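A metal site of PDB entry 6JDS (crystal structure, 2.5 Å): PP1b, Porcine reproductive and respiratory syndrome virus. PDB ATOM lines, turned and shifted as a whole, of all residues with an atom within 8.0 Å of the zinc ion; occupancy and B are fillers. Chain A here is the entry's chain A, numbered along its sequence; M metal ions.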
ATOM      1  N   ILE A  39     -20.775 -33.794  -6.169  1.00  0.00           N
ATOM      2  CA  ILE A  39     -20.977 -32.616  -5.322  1.00  0.00           C
ATOM      3  C   ILE A  39     -22.175 -31.777  -5.785  1.00  0.00           C
ATOM      4  O   ILE A  39     -22.914 -32.178  -6.680  1.00  0.00           O
ATOM      5  CB  ILE A  39     -19.679 -31.778  -5.211  1.00  0.00           C
ATOM      6  CG1 ILE A  39     -19.216 -31.268  -6.570  1.00  0.00           C
ATOM      7  CG2 ILE A  39     -18.575 -32.597  -4.558  1.00  0.00           C
ATOM      8  CD1 ILE A  39     -18.113 -30.230  -6.487  1.00  0.00           C
ATOM      9  N   TRP A  40     -22.359 -30.622  -5.139  1.00  0.00           N
ATOM     10  CA  TRP A  40     -23.482 -29.700  -5.384  1.00  0.00           C
ATOM     11  C   TRP A  40     -23.822 -29.385  -6.848  1.00  0.00           C
ATOM     12  O   TRP A  40     -24.981 -29.128  -7.148  1.00  0.00           O
ATOM     13  CB  TRP A  40     -23.277 -28.384  -4.605  1.00  0.00           C
ATOM     14  CG  TRP A  40     -21.924 -27.735  -4.750  1.00  0.00           C
ATOM     15  CD1 TRP A  40     -21.582 -26.744  -5.622  1.00  0.00           C
ATOM     16  CD2 TRP A  40     -20.746 -28.017  -3.986  1.00  0.00           C
ATOM     17  NE1 TRP A  40     -20.267 -26.389  -5.452  1.00  0.00           N
ATOM     18  CE2 TRP A  40     -19.722 -27.156  -4.456  1.00  0.00           C
ATOM     19  CE3 TRP A  40     -20.441 -28.919  -2.953  1.00  0.00           C
ATOM     20  CZ2 TRP A  40     -18.430 -27.173  -3.934  1.00  0.00           C
ATOM     21  CZ3 TRP A  40     -19.153 -28.928  -2.429  1.00  0.00           C
ATOM     22  CH2 TRP A  40     -18.167 -28.070  -2.926  1.00  0.00           C
ATOM     23  N   CYS A  41     -22.828 -29.407  -7.738  1.00  0.00           N
ATOM     24  CA  CYS A  41     -23.079 -29.154  -9.163  1.00  0.00           C
ATOM     25  C   CYS A  41     -23.490 -30.396  -9.952  1.00  0.00           C
ATOM     26  O   CYS A  41     -23.810 -30.292 -11.133  1.00  0.00           O
ATOM     27  CB  CYS A  41     -21.846 -28.519  -9.796  1.00  0.00           C
ATOM     28  SG  CYS A  41     -20.334 -29.489  -9.594  1.00  0.00           S
ATOM     29  N   GLY A  42     -23.454 -31.569  -9.313  1.00  0.00           N
ATOM     30  CA  GLY A  42     -23.862 -32.825  -9.949  1.00  0.00           C
ATOM     31  C   GLY A  42     -22.729 -33.608 -10.593  1.00  0.00           C
ATOM     32  O   GLY A  42     -22.941 -34.717 -11.073  1.00  0.00           O
ATOM     33  N   HIS A  43     -21.526 -33.032 -10.590  1.00  0.00           N
ATOM     34  CA  HIS A  43     -20.359 -33.663 -11.213  1.00  0.00           C
ATOM     35  C   HIS A  43     -19.377 -34.106 -10.131  1.00  0.00           C
ATOM     36  O   HIS A  43     -19.460 -33.650  -8.990  1.00  0.00           O
ATOM     37  CB  HIS A  43     -19.670 -32.668 -12.152  1.00  0.00           C
ATOM     38  CG  HIS A  43     -20.607 -31.975 -13.083  1.00  0.00           C
ATOM     39  ND1 HIS A  43     -20.718 -30.598 -13.151  1.00  0.00           N
ATOM     40  CD2 HIS A  43     -21.485 -32.458 -13.996  1.00  0.00           C
ATOM     41  CE1 HIS A  43     -21.614 -30.276 -14.065  1.00  0.00           C
ATOM     42  NE2 HIS A  43     -22.091 -31.381 -14.590  1.00  0.00           N
ATOM     43  N   PRO A  44     -18.442 -35.013 -10.479  1.00  0.00           N
ATOM     44  CA  PRO A  44     -17.409 -35.387  -9.508  1.00  0.00           C
ATOM     45  C   PRO A  44     -16.515 -34.197  -9.166  1.00  0.00           C
ATOM     46  O   PRO A  44     -16.202 -33.383 -10.034  1.00  0.00           O
ATOM     47  CB  PRO A  44     -16.608 -36.471 -10.240  1.00  0.00           C
ATOM     48  CG  PRO A  44     -17.508 -36.959 -11.324  1.00  0.00           C
ATOM     49  CD  PRO A  44     -18.347 -35.788 -11.728  1.00  0.00           C
ATOM     50  N   ALA A  45     -16.116 -34.092  -7.891  1.00  0.00           N
ATOM     51  CA  ALA A  45     -15.277 -32.985  -7.442  1.00  0.00           C
ATOM     52  C   ALA A  45     -13.928 -33.008  -8.160  1.00  0.00           C
ATOM     53  O   ALA A  45     -13.328 -34.068  -8.331  1.00  0.00           O
ATOM     54  CB  ALA A  45     -15.068 -33.057  -5.936  1.00  0.00           C
ATOM     55  N   GLY A  46     -13.483 -31.840  -8.611  1.00  0.00           N
ATOM     56  CA  GLY A  46     -12.222 -31.724  -9.337  1.00  0.00           C
ATOM     57  C   GLY A  46     -12.208 -32.297 -10.745  1.00  0.00           C
ATOM     58  O   GLY A  46     -11.140 -32.432 -11.352  1.00  0.00           O
ATOM     59  N   SER A  47     -13.379 -32.637 -11.278  1.00  0.00           N
ATOM     60  CA  SER A  47     -13.476 -33.198 -12.634  1.00  0.00           C
ATOM     61  C   SER A  47     -13.312 -32.119 -13.696  1.00  0.00           C
ATOM     62  O   SER A  47     -12.885 -32.406 -14.811  1.00  0.00           O
ATOM     63  CB  SER A  47     -14.826 -33.890 -12.821  1.00  0.00           C
ATOM     64  OG  SER A  47     -15.888 -32.963 -12.776  1.00  0.00           O
ATOM     65  N   GLY A  48     -13.676 -30.882 -13.355  1.00  0.00           N
ATOM     66  CA  GLY A  48     -13.626 -29.771 -14.299  1.00  0.00           C
ATOM     67  C   GLY A  48     -14.791 -29.754 -15.273  1.00  0.00           C
ATOM     68  O   GLY A  48     -14.716 -29.128 -16.323  1.00  0.00           O
ATOM     69  N   SER A  49     -15.874 -30.454 -14.927  1.00  0.00           N
ATOM     70  CA  SER A  49     -17.061 -30.506 -15.774  1.00  0.00           C
ATOM     71  C   SER A  49     -17.786 -29.161 -15.840  1.00  0.00           C
ATOM     72  O   SER A  49     -18.442 -28.846 -16.827  1.00  0.00           O
ATOM     73  CB  SER A  49     -18.016 -31.588 -15.278  1.00  0.00           C
ATOM     74  OG  SER A  49     -17.406 -32.866 -15.294  1.00  0.00           O
ATOM     75  N   CYS A  50     -17.669 -28.381 -14.759  1.00  0.00           N
ATOM     76  CA  CYS A  50     -18.194 -27.025 -14.732  1.00  0.00           C
ATOM     77  C   CYS A  50     -17.326 -26.181 -13.804  1.00  0.00           C
ATOM     78  O   CYS A  50     -16.384 -26.689 -13.201  1.00  0.00           O
ATOM     79  CB  CYS A  50     -19.666 -27.010 -14.282  1.00  0.00           C
ATOM     80  SG  CYS A  50     -19.958 -27.134 -12.503  1.00  0.00           S
ATOM     81  N   SER A  51     -17.656 -24.898 -13.687  1.00  0.00           N
ATOM     82  CA  SER A  51     -16.922 -23.976 -12.830  1.00  0.00           C
ATOM     83  C   SER A  51     -16.770 -24.459 -11.381  1.00  0.00           C
ATOM     84  O   SER A  51     -15.712 -24.295 -10.783  1.00  0.00           O
ATOM     85  CB  SER A  51     -17.600 -22.593 -12.838  1.00  0.00           C
ATOM     86  OG  SER A  51     -16.977 -21.706 -11.932  1.00  0.00           O
ATOM     87  N   GLU A  52     -17.824 -25.062 -10.841  1.00  0.00           N
ATOM     88  CA  GLU A  52     -17.851 -25.461  -9.437  1.00  0.00           C
ATOM     89  C   GLU A  52     -16.956 -26.657  -9.114  1.00  0.00           C
ATOM     90  O   GLU A  52     -16.427 -26.751  -8.006  1.00  0.00           O
ATOM     91  CB  GLU A  52     -19.279 -25.745  -8.982  1.00  0.00           C
ATOM     92  CG  GLU A  52     -20.139 -24.488  -8.891  1.00  0.00           C
ATOM     93  CD  GLU A  52     -19.629 -23.514  -7.843  1.00  0.00           C
ATOM     94  OE1 GLU A  52     -19.260 -23.959  -6.730  1.00  0.00           O
ATOM     95  OE2 GLU A  52     -19.617 -22.298  -8.122  1.00  0.00           O
ATOM     96  N   CYS A  53     -16.798 -27.578 -10.058  1.00  0.00           N
ATOM     97  CA  CYS A  53     -15.904 -28.727  -9.870  1.00  0.00           C
ATOM     98  C   CYS A  53     -14.550 -28.553 -10.579  1.00  0.00           C
ATOM     99  O   CYS A  53     -13.875 -29.541 -10.868  1.00  0.00           O
ATOM    100  CB  CYS A  53     -16.599 -30.008 -10.322  1.00  0.00           C
ATOM    101  SG  CYS A  53     -17.188 -29.969 -12.022  1.00  0.00           S
ATOM    102  N   GLU A  54     -14.156 -27.306 -10.851  1.00  0.00           N
ATOM    103  CA  GLU A  54     -12.823 -27.011 -11.399  1.00  0.00           C
ATOM    104  C   GLU A  54     -11.684 -27.074 -10.368  1.00  0.00           C
ATOM    105  O   GLU A  54     -10.595 -27.534 -10.699  1.00  0.00           O
ATOM    106  CB  GLU A  54     -12.800 -25.647 -12.097  1.00  0.00           C
ATOM    107  CG  GLU A  54     -13.218 -25.683 -13.565  1.00  0.00           C
ATOM    108  CD  GLU A  54     -13.450 -24.304 -14.148  1.00  0.00           C
ATOM    109  OE1 GLU A  54     -12.987 -23.298 -13.556  1.00  0.00           O
ATOM    110  OE2 GLU A  54     -14.105 -24.204 -15.219  1.00  0.00           O
ATOM    111  N   PRO A  55     -11.932 -26.587  -9.128  1.00  0.00           N
ATOM    112  CA  PRO A  55     -10.851 -26.605  -8.135  1.00  0.00           C
ATOM    113  C   PRO A  55     -10.236 -27.988  -7.927  1.00  0.00           C
ATOM    114  O   PRO A  55     -10.972 -28.976  -7.886  1.00  0.00           O
ATOM    115  CB  PRO A  55     -11.543 -26.123  -6.851  1.00  0.00           C
ATOM    116  CG  PRO A  55     -12.676 -25.292  -7.328  1.00  0.00           C
ATOM    117  CD  PRO A  55     -13.138 -25.910  -8.623  1.00  0.00           C
HETATM  118 ZN    ZN M   1     -19.393 -29.295 -11.809  1.00  0.00          ZN
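The zinc ion is bound by ND1 of His 43 (2.3 Å).
The side-chain sulfur (SG) of Cys 53 binds the zinc ion (2.3 Å).
SG of Cys 50 binds the zinc ion.
SG of Cys 41 is bound to the zinc ion, at 2.4 Å.
The zinc ion has four donor atoms within binding distance.
The backbone NH (N) of Gly 46 lies close to the backbone carbonyl oxygen (O) of Cys 53 (3.2 Å).
The side-chain sulfur (SG) of Cys 53 sits close to the backbone NH (N) of Ser 49.
The backbone carbonyl oxygen (O) of Cys 53 is in hydrogen-bond range of the backbone NH (N) of Gly 48 (2.8 Å).
O of Cys 53 is in hydrogen-bond range of N of Ser 47 (3.2 Å).
The backbone NH of Glu 52 sits close to the side-chain sulfur of Cys 50 (3.4 Å).
Four residues have an atom within 4 Å of the zinc ion: Cys 41, His 43, Cys 50 and Cys 53.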
